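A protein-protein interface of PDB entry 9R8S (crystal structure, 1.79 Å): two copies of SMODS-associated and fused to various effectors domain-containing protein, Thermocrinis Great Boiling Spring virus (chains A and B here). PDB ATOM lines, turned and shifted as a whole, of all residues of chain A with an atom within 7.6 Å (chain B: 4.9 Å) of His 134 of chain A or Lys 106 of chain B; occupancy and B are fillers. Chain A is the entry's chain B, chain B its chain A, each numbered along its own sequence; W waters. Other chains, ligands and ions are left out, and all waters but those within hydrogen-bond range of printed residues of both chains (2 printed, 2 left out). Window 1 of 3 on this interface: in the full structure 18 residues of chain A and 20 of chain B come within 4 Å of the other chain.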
ATOM      1  N   ASN A 131       7.037  11.402 -22.429  1.00  0.00           N
ATOM      2  CA  ASN A 131       7.687  10.646 -23.486  1.00  0.00           C
ATOM      3  C   ASN A 131       8.344  11.656 -24.431  1.00  0.00           C
ATOM      4  O   ASN A 131       7.835  11.911 -25.516  1.00  0.00           O
ATOM      5  CB  ASN A 131       6.636   9.740 -24.109  1.00  0.00           C
ATOM      6  CG  ASN A 131       7.196   8.550 -24.842  1.00  0.00           C
ATOM      7  OD1 ASN A 131       8.368   8.185 -24.683  1.00  0.00           O
ATOM      8  ND2 ASN A 131       6.351   7.908 -25.628  1.00  0.00           N
ATOM      9  N   TYR A 132       9.452  12.256 -23.978  1.00  0.00           N
ATOM     10  CA  TYR A 132       9.979  13.480 -24.552  1.00  0.00           C
ATOM     11  C   TYR A 132      11.305  13.236 -25.270  1.00  0.00           C
ATOM     12  O   TYR A 132      11.708  14.062 -26.085  1.00  0.00           O
ATOM     13  CB  TYR A 132      10.206  14.537 -23.465  1.00  0.00           C
ATOM     14  CG  TYR A 132       8.958  15.178 -22.864  1.00  0.00           C
ATOM     15  CD1 TYR A 132       7.675  14.790 -23.234  1.00  0.00           C
ATOM     16  CD2 TYR A 132       9.069  16.154 -21.879  1.00  0.00           C
ATOM     17  CE1 TYR A 132       6.551  15.380 -22.682  1.00  0.00           C
ATOM     18  CE2 TYR A 132       7.954  16.742 -21.310  1.00  0.00           C
ATOM     19  CZ  TYR A 132       6.690  16.354 -21.709  1.00  0.00           C
ATOM     20  OH  TYR A 132       5.593  16.944 -21.157  1.00  0.00           O
ATOM     21  N   SER A 133      12.012  12.152 -24.932  1.00  0.00           N
ATOM     22  CA  SER A 133      13.383  11.981 -25.390  1.00  0.00           C
ATOM     23  C   SER A 133      13.444  10.850 -26.415  1.00  0.00           C
ATOM     24  O   SER A 133      12.404  10.354 -26.857  1.00  0.00           O
ATOM     25  CB  SER A 133      14.330  11.803 -24.237  1.00  0.00           C
ATOM     26  OG  SER A 133      14.411  13.029 -23.510  1.00  0.00           O
ATOM     27  N   HIS A 134      14.668  10.479 -26.807  1.00  0.00           N
ATOM     28  CA  HIS A 134      14.879   9.549 -27.903  1.00  0.00           C
ATOM     29  C   HIS A 134      14.236   8.194 -27.616  1.00  0.00           C
ATOM     30  O   HIS A 134      13.582   7.628 -28.485  1.00  0.00           O
ATOM     31  CB  HIS A 134      16.381   9.392 -28.178  1.00  0.00           C
ATOM     32  CG  HIS A 134      16.678   8.452 -29.296  1.00  0.00           C
ATOM     33  ND1 HIS A 134      16.420   8.767 -30.615  1.00  0.00           N
ATOM     34  CD2 HIS A 134      17.164   7.197 -29.293  1.00  0.00           C
ATOM     35  CE1 HIS A 134      16.774   7.731 -31.372  1.00  0.00           C
ATOM     36  NE2 HIS A 134      17.219   6.763 -30.596  1.00  0.00           N
ATOM     37  N   HIS A 135      14.404   7.701 -26.377  1.00  0.00           N
ATOM     38  CA  HIS A 135      13.984   6.355 -26.033  1.00  0.00           C
ATOM     39  C   HIS A 135      12.477   6.326 -25.787  1.00  0.00           C
ATOM     40  O   HIS A 135      11.948   7.128 -25.019  1.00  0.00           O
ATOM     41  CB  HIS A 135      14.836   5.807 -24.877  1.00  0.00           C
ATOM     42  CG  HIS A 135      16.232   5.540 -25.310  1.00  0.00           C
ATOM     43  ND1 HIS A 135      17.238   6.479 -25.253  1.00  0.00           N
ATOM     44  CD2 HIS A 135      16.775   4.455 -25.872  1.00  0.00           C
ATOM     45  CE1 HIS A 135      18.358   5.958 -25.749  1.00  0.00           C
ATOM     46  NE2 HIS A 135      18.100   4.729 -26.137  1.00  0.00           N
ATOM     47  N   GLU A 136      11.804   5.389 -26.473  1.00  0.00           N
ATOM     48  CA  GLU A 136      10.355   5.259 -26.456  1.00  0.00           C
ATOM     49  C   GLU A 136       9.938   4.395 -25.266  1.00  0.00           C
ATOM     50  O   GLU A 136      10.435   3.284 -25.153  1.00  0.00           O
ATOM     51  CB  GLU A 136       9.960   4.600 -27.779  1.00  0.00           C
ATOM     52  CG  GLU A 136       8.497   4.188 -27.863  1.00  0.00           C
ATOM     53  CD  GLU A 136       7.541   5.337 -27.628  1.00  0.00           C
ATOM     54  OE1 GLU A 136       7.727   6.399 -28.257  1.00  0.00           O
ATOM     55  OE2 GLU A 136       6.597   5.150 -26.843  1.00  0.00           O
ATOM     56  N   ILE A 137       9.041   4.895 -24.397  1.00  0.00           N
ATOM     57  CA  ILE A 137       8.798   4.233 -23.121  1.00  0.00           C
ATOM     58  C   ILE A 137       7.352   3.785 -22.928  1.00  0.00           C
ATOM     59  O   ILE A 137       7.105   3.127 -21.928  1.00  0.00           O
ATOM     60  CB  ILE A 137       9.215   5.113 -21.928  1.00  0.00           C
ATOM     61  CG1 ILE A 137       8.363   6.381 -21.815  1.00  0.00           C
ATOM     62  CG2 ILE A 137      10.715   5.399 -21.979  1.00  0.00           C
ATOM     63  CD1 ILE A 137       8.500   7.110 -20.487  1.00  0.00           C
ATOM     64  N   ILE A 164       9.949  17.993 -31.746  1.00  0.00           N
ATOM     65  CA  ILE A 164      11.245  18.171 -31.095  1.00  0.00           C
ATOM     66  C   ILE A 164      11.635  16.977 -30.220  1.00  0.00           C
ATOM     67  O   ILE A 164      12.662  17.047 -29.547  1.00  0.00           O
ATOM     68  CB  ILE A 164      11.276  19.466 -30.263  1.00  0.00           C
ATOM     69  CG1 ILE A 164      10.254  19.403 -29.124  1.00  0.00           C
ATOM     70  CG2 ILE A 164      11.069  20.673 -31.165  1.00  0.00           C
ATOM     71  CD1 ILE A 164      10.295  20.572 -28.162  1.00  0.00           C
ATOM     72  N   THR A 165      10.843  15.900 -30.245  1.00  0.00           N
ATOM     73  CA  THR A 165      11.143  14.698 -29.467  1.00  0.00           C
ATOM     74  C   THR A 165      12.569  14.231 -29.766  1.00  0.00           C
ATOM     75  O   THR A 165      12.940  14.011 -30.921  1.00  0.00           O
ATOM     76  CB  THR A 165      10.134  13.587 -29.762  1.00  0.00           C
ATOM     77  OG1 THR A 165       8.831  14.064 -29.446  1.00  0.00           O
ATOM     78  CG2 THR A 165      10.371  12.336 -28.935  1.00  0.00           C
ATOM     79  N   GLY A 166      13.379  14.112 -28.706  1.00  0.00           N
ATOM     80  CA  GLY A 166      14.729  13.584 -28.803  1.00  0.00           C
ATOM     81  C   GLY A 166      15.789  14.636 -29.142  1.00  0.00           C
ATOM     82  O   GLY A 166      16.980  14.322 -29.162  1.00  0.00           O
ATOM     83  N   ASN A 167      15.364  15.874 -29.422  1.00  0.00           N
ATOM     84  CA  ASN A 167      16.283  16.933 -29.788  1.00  0.00           C
ATOM     85  C   ASN A 167      15.722  18.254 -29.280  1.00  0.00           C
ATOM     86  O   ASN A 167      15.292  19.094 -30.061  1.00  0.00           O
ATOM     87  CB  ASN A 167      16.543  16.935 -31.297  1.00  0.00           C
ATOM     88  CG  ASN A 167      17.503  18.022 -31.727  1.00  0.00           C
ATOM     89  OD1 ASN A 167      18.279  18.548 -30.917  1.00  0.00           O
ATOM     90  ND2 ASN A 167      17.484  18.362 -33.006  1.00  0.00           N
ATOM     91  N   SER A 201      10.909   9.880 -19.753  1.00  0.00           N
ATOM     92  CA  SER A 201      11.940   9.854 -20.797  1.00  0.00           C
ATOM     93  C   SER A 201      12.188  11.304 -21.205  1.00  0.00           C
ATOM     94  O   SER A 201      11.538  11.806 -22.109  1.00  0.00           O
ATOM     95  CB  SER A 201      11.526   9.012 -22.004  1.00  0.00           C
ATOM     96  OG  SER A 201      12.389   9.168 -23.131  1.00  0.00           O
ATOM     97  N   CYS A 202      13.045  12.006 -20.455  1.00  0.00           N
ATOM     98  CA  CYS A 202      12.919  13.445 -20.317  1.00  0.00           C
ATOM     99  C   CYS A 202      14.250  14.043 -19.876  1.00  0.00           C
ATOM    100  O   CYS A 202      14.912  13.499 -18.978  1.00  0.00           O
ATOM    101  CB  CYS A 202      11.755  13.664 -19.356  1.00  0.00           C
ATOM    102  SG  CYS A 202      11.571  15.339 -18.733  1.00  0.00           S
ATOM    103  N   PRO A 203      14.710  15.156 -20.501  1.00  0.00           N
ATOM    104  CA  PRO A 203      15.906  15.851 -20.040  1.00  0.00           C
ATOM    105  C   PRO A 203      15.800  16.305 -18.587  1.00  0.00           C
ATOM    106  O   PRO A 203      14.724  16.689 -18.131  1.00  0.00           O
ATOM    107  CB  PRO A 203      16.033  17.038 -20.983  1.00  0.00           C
ATOM    108  CG  PRO A 203      15.270  16.599 -22.210  1.00  0.00           C
ATOM    109  CD  PRO A 203      14.137  15.778 -21.699  1.00  0.00           C
ATOM    110  N   SER B  80      26.311   9.765 -25.941  1.00  0.00           N
ATOM    111  CA  SER B  80      25.787  10.815 -26.795  1.00  0.00           C
ATOM    112  C   SER B  80      25.972  12.202 -26.174  1.00  0.00           C
ATOM    113  O   SER B  80      25.207  13.103 -26.467  1.00  0.00           O
ATOM    114  CB  SER B  80      24.354  10.523 -27.163  1.00  0.00           C
ATOM    115  OG  SER B  80      23.563  10.235 -26.023  1.00  0.00           O
ATOM    116  N   VAL B 102      24.929  16.184 -31.560  1.00  0.00           N
ATOM    117  CA  VAL B 102      24.669  14.752 -31.466  1.00  0.00           C
ATOM    118  C   VAL B 102      23.157  14.502 -31.382  1.00  0.00           C
ATOM    119  O   VAL B 102      22.670  13.506 -31.898  1.00  0.00           O
ATOM    120  CB  VAL B 102      25.430  14.098 -30.288  1.00  0.00           C
ATOM    121  CG1 VAL B 102      25.092  12.616 -30.117  1.00  0.00           C
ATOM    122  CG2 VAL B 102      26.933  14.220 -30.444  1.00  0.00           C
ATOM    123  N   ARG B 103      22.409  15.428 -30.769  1.00  0.00           N
ATOM    124  CA  ARG B 103      20.971  15.271 -30.610  1.00  0.00           C
ATOM    125  C   ARG B 103      20.265  15.242 -31.964  1.00  0.00           C
ATOM    126  O   ARG B 103      19.180  14.657 -32.067  1.00  0.00           O
ATOM    127  CB  ARG B 103      20.386  16.338 -29.679  1.00  0.00           C
ATOM    128  CG  ARG B 103      20.685  16.029 -28.222  1.00  0.00           C
ATOM    129  CD  ARG B 103      20.187  17.136 -27.311  1.00  0.00           C
ATOM    130  NE  ARG B 103      20.967  18.374 -27.467  1.00  0.00           N
ATOM    131  CZ  ARG B 103      20.597  19.493 -28.098  1.00  0.00           C
ATOM    132  NH1 ARG B 103      19.443  19.572 -28.733  1.00  0.00           N
ATOM    133  NH2 ARG B 103      21.406  20.541 -28.115  1.00  0.00           N
ATOM    134  N   ALA B 104      20.877  15.824 -33.008  1.00  0.00           N
ATOM    135  CA  ALA B 104      20.289  15.767 -34.339  1.00  0.00           C
ATOM    136  C   ALA B 104      20.158  14.325 -34.834  1.00  0.00           C
ATOM    137  O   ALA B 104      19.243  14.033 -35.605  1.00  0.00           O
ATOM    138  CB  ALA B 104      21.074  16.626 -35.308  1.00  0.00           C
ATOM    139  N   LEU B 105      21.041  13.425 -34.362  1.00  0.00           N
ATOM    140  CA  LEU B 105      20.965  12.007 -34.705  1.00  0.00           C
ATOM    141  C   LEU B 105      19.853  11.290 -33.944  1.00  0.00           C
ATOM    142  O   LEU B 105      19.477  10.186 -34.333  1.00  0.00           O
ATOM    143  CB  LEU B 105      22.291  11.303 -34.437  1.00  0.00           C
ATOM    144  CG  LEU B 105      23.481  11.722 -35.305  1.00  0.00           C
ATOM    145  CD1 LEU B 105      24.719  10.988 -34.824  1.00  0.00           C
ATOM    146  CD2 LEU B 105      23.267  11.482 -36.796  1.00  0.00           C
ATOM    147  N   LYS B 106      19.354  11.878 -32.845  1.00  0.00           N
ATOM    148  CA  LYS B 106      18.412  11.208 -31.959  1.00  0.00           C
ATOM    149  C   LYS B 106      17.002  11.780 -32.079  1.00  0.00           C
ATOM    150  O   LYS B 106      16.090  11.342 -31.389  1.00  0.00           O
ATOM    151  CB  LYS B 106      18.923  11.330 -30.518  1.00  0.00           C
ATOM    152  CG  LYS B 106      20.180  10.514 -30.289  1.00  0.00           C
ATOM    153  CD  LYS B 106      20.821  10.663 -28.911  1.00  0.00           C
ATOM    154  CE  LYS B 106      19.937  10.194 -27.830  1.00  0.00           C
ATOM    155  NZ  LYS B 106      20.699  10.098 -26.580  1.00  0.00           N
ATOM    156  N   GLN B 107      16.838  12.774 -32.951  1.00  0.00           N
ATOM    157  CA  GLN B 107      15.543  13.377 -33.215  1.00  0.00           C
ATOM    158  C   GLN B 107      14.556  12.306 -33.679  1.00  0.00           C
ATOM    159  O   GLN B 107      14.853  11.545 -34.591  1.00  0.00           O
ATOM    160  CB  GLN B 107      15.858  14.425 -34.278  1.00  0.00           C
ATOM    161  CG  GLN B 107      14.652  14.956 -35.034  1.00  0.00           C
ATOM    162  CD  GLN B 107      14.073  16.174 -34.378  1.00  0.00           C
ATOM    163  OE1 GLN B 107      14.686  17.252 -34.388  1.00  0.00           O
ATOM    164  NE2 GLN B 107      12.877  15.998 -33.835  1.00  0.00           N
ATOM    165  N   ARG B 108      13.381  12.238 -33.050  1.00  0.00           N
ATOM    166  CA  ARG B 108      12.384  11.243 -33.428  1.00  0.00           C
ATOM    167  C   ARG B 108      11.486  11.836 -34.512  1.00  0.00           C
ATOM    168  O   ARG B 108      11.134  12.999 -34.425  1.00  0.00           O
ATOM    169  CB  ARG B 108      11.580  10.788 -32.210  1.00  0.00           C
ATOM    170  CG  ARG B 108      12.397   9.996 -31.198  1.00  0.00           C
ATOM    171  CD  ARG B 108      12.524   8.525 -31.568  1.00  0.00           C
ATOM    172  NE  ARG B 108      11.234   7.832 -31.637  1.00  0.00           N
ATOM    173  CZ  ARG B 108      10.454   7.572 -30.582  1.00  0.00           C
ATOM    174  NH1 ARG B 108      10.898   7.796 -29.350  1.00  0.00           N
ATOM    175  NH2 ARG B 108       9.257   7.041 -30.766  1.00  0.00           N
ATOM    176  N   ASN B 178      19.858   8.790 -38.593  1.00  0.00           N
ATOM    177  CA  ASN B 178      18.794   9.390 -37.798  1.00  0.00           C
ATOM    178  C   ASN B 178      17.479   8.639 -38.018  1.00  0.00           C
ATOM    179  O   ASN B 178      16.794   8.277 -37.065  1.00  0.00           O
ATOM    180  CB  ASN B 178      18.658  10.883 -38.093  1.00  0.00           C
ATOM    181  CG  ASN B 178      17.499  11.537 -37.370  1.00  0.00           C
ATOM    182  OD1 ASN B 178      16.740  12.292 -37.989  1.00  0.00           O
ATOM    183  ND2 ASN B 178      17.344  11.281 -36.072  1.00  0.00           N
ATOM    184  N   SER B 181      17.594   5.126 -36.471  1.00  0.00           N
ATOM    185  CA  SER B 181      17.526   5.210 -35.014  1.00  0.00           C
ATOM    186  C   SER B 181      16.098   5.467 -34.556  1.00  0.00           C
ATOM    187  O   SER B 181      15.638   4.850 -33.592  1.00  0.00           O
ATOM    188  CB  SER B 181      18.463   6.258 -34.500  1.00  0.00           C
ATOM    189  OG  SER B 181      19.806   5.915 -34.846  1.00  0.00           O
ATOM    190  N   SER B 182      15.404   6.379 -35.252  1.00  0.00           N
ATOM    191  CA  SER B 182      14.029   6.727 -34.923  1.00  0.00           C
ATOM    192  C   SER B 182      13.099   5.527 -35.121  1.00  0.00           C
ATOM    193  O   SER B 182      12.195   5.313 -34.326  1.00  0.00           O
ATOM    194  CB  SER B 182      13.580   7.940 -35.699  1.00  0.00           C
ATOM    195  OG  SER B 182      12.248   8.315 -35.409  1.00  0.00           O
ATOM    196  N   GLN B 185      13.263   3.024 -32.248  1.00  0.00           N
ATOM    197  CA  GLN B 185      12.460   3.403 -31.092  1.00  0.00           C
ATOM    198  C   GLN B 185      10.977   3.255 -31.433  1.00  0.00           C
ATOM    199  O   GLN B 185      10.209   2.804 -30.610  1.00  0.00           O
ATOM    200  CB  GLN B 185      12.851   4.806 -30.614  1.00  0.00           C
ATOM    201  CG  GLN B 185      14.310   4.928 -30.172  1.00  0.00           C
ATOM    202  CD  GLN B 185      14.686   3.944 -29.079  1.00  0.00           C
ATOM    203  OE1 GLN B 185      13.924   3.715 -28.130  1.00  0.00           O
ATOM    204  NE2 GLN B 185      15.859   3.341 -29.199  1.00  0.00           N
ATOM    205  N   ALA B 213      23.064   6.470 -30.983  1.00  0.00           N
ATOM    206  CA  ALA B 213      21.687   6.831 -30.667  1.00  0.00           C
ATOM    207  C   ALA B 213      21.013   5.747 -29.818  1.00  0.00           C
ATOM    208  O   ALA B 213      20.354   6.042 -28.816  1.00  0.00           O
ATOM    209  CB  ALA B 213      20.904   7.087 -31.954  1.00  0.00           C
ATOM    210  N   PHE B 214      21.176   4.483 -30.216  1.00  0.00           N
ATOM    211  CA  PHE B 214      20.442   3.394 -29.590  1.00  0.00           C
ATOM    212  C   PHE B 214      20.919   3.212 -28.148  1.00  0.00           C
ATOM    213  O   PHE B 214      20.108   3.020 -27.233  1.00  0.00           O
ATOM    214  CB  PHE B 214      20.614   2.100 -30.388  1.00  0.00           C
ATOM    215  CG  PHE B 214      19.663   1.004 -29.944  1.00  0.00           C
ATOM    216  CD1 PHE B 214      18.377   0.958 -30.452  1.00  0.00           C
ATOM    217  CD2 PHE B 214      20.054   0.018 -29.046  1.00  0.00           C
ATOM    218  CE1 PHE B 214      17.489  -0.026 -30.049  1.00  0.00           C
ATOM    219  CE2 PHE B 214      19.167  -0.976 -28.653  1.00  0.00           C
ATOM    220  CZ  PHE B 214      17.885  -0.988 -29.138  1.00  0.00           C
HETATM  221  O   HOH W   1      17.496   4.207 -31.584  1.00  0.00           O
HETATM  222  O   HOH W   2      17.426   1.727 -27.248  1.00  0.00           O
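Of the 14 printed residues of chain A, 8 touch a printed residue of chain B.
Printed residues of chain A that touch a printed residue of chain B: Ser 133, His 134, His 135, Glu 136, Ile 164, Thr 165, Gly 166 and Asn 167.
Hydrophobic or aromatic side chains of chain A that line the printed part of chain B: His 134 and His 135.
Among the printed residues, Asp or Glu carboxylates within 4 Å of a Lys or Arg side-chain nitrogen of the other chain: Glu 136 of chain A with Arg 108 of chain B (3.0 Å).
O of Ser 133 of chain A touches NH1 of Arg 108 of chain B (3.9 Å).
His 134 of chain A touches Ser 181 of chain B.
His 134 of chain A touches Gln 185 of chain B (O to CG, 3.3 Å).
Ala 213 of chain B touches His 134 of chain A.
CA of His 135 of chain A touches OE1 of Gln 185 of chain B, 3.4 Å away.
CE1 of His 135 of chain A touches O of Ala 213 of chain B, 3.7 Å away.
NE2 of Gln 107 of chain B touches CA of Ile 164 of chain A (3.9 Å).
CA of Gln 107 of chain B touches O of Thr 165 of chain A, 3.5 Å away.
O of Gly 166 of chain A touches O of Arg 103 of chain B (3.7 Å).
Gly 166 of chain A touches Lys 106 of chain B.
ND1 of His 134 of chain A lies within hydrogen-bond range of O of Lys 106 of chain B (2.7 Å).
O of Thr 165 of chain A lies within hydrogen-bond range of N of Arg 108 of chain B (2.8 Å).
A ring nitrogen (NE2) of His 135 of chain A lies within hydrogen-bond range of the backbone carbonyl oxygen of Phe 214 of chain B (2.9 Å).
NH2 of Arg 108 of chain B is in salt-bridge range of OE1 of Glu 136 of chain A (3.0 Å).
NH1 of Arg 103 of chain B sits at hydrogen-bond distance from OD1 of Asn 167 of chain A (2.7 Å).
The backbone NH (N) of Glu 136 of chain A is in hydrogen-bond range of the side-chain amide oxygen (OE1) of Gln 185 of chain B (3.2 Å).
OE1 of Gln 107 of chain B is in hydrogen-bond range of ND2 of Asn 167 of chain A, at 3.3 Å.
NH1 of Arg 108 of chain B is in hydrogen-bond range of O of His 134 of chain A.
ND2 of Asn 131 of chain A sits at hydrogen-bond distance from OE2 of Glu 136 of chain A, 3.0 Å away.
OG of Ser 133 of chain A lies within hydrogen-bond range of N of Cys 202 of chain A (3.5 Å).
The backbone carbonyl oxygen of Gln 107 of chain B is in hydrogen-bond range of the side-chain amide nitrogen of Asn 178 of chain B (2.9 Å).
The backbone carbonyl oxygen of His 135 of chain A lies within hydrogen-bond range of the side-chain hydroxyl of Ser 201 of chain A (2.8 Å).
OG of Ser 80 of chain B is in hydrogen-bond range of NZ of Lys 106 of chain B.
O of Ser 201 of chain A sits at hydrogen-bond distance from N of Ser 133 of chain A (2.9 Å).
Of chain B, only Lys 106 (2.7 Å), Arg 108 (2.8 Å), Ser 181 (3.8 Å), Gln 185 (3.3 Å) and Ala 213 (3.4 Å) come within 4 Å of His 134 of chain A.
Cys 202 of chain A touches none of the printed residues of chain B.
Pro 203 of chain A touches none of the printed residues of chain B.
Of the printed residues of chain A, Lys 106 of chain B touches His 134 and Gly 166.
Of the printed residues of chain A, Gln 107 of chain B touches Ile 164 (3.9 Å), Thr 165 (3.5 Å) and Asn 167 (3.3 Å).
Of the printed residues of chain A, Ser 181 of chain B touches His 134.
The nearest residue of chain A that does not touch Lys 106 of chain B is Thr 165 of chain A (4.2 Å).
The nearest printed residue of chain A that does not touch Ser 181 of chain B is His 135 of chain A (7.8 Å).
No position is printed for both chains.
Water W1 lies within hydrogen-bond range of NE2 of His 134 of chain A (2.8 Å), O of Ser 181 of chain B (2.8 Å) and NE2 of Gln 185 of chain B (3.0 Å).
Water W2 lies within hydrogen-bond range of O of Phe 214 of chain B (3.0 Å), NE2 of Gln 185 of chain B (3.0 Å) and NE2 of His 135 of chain A (3.3 Å).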
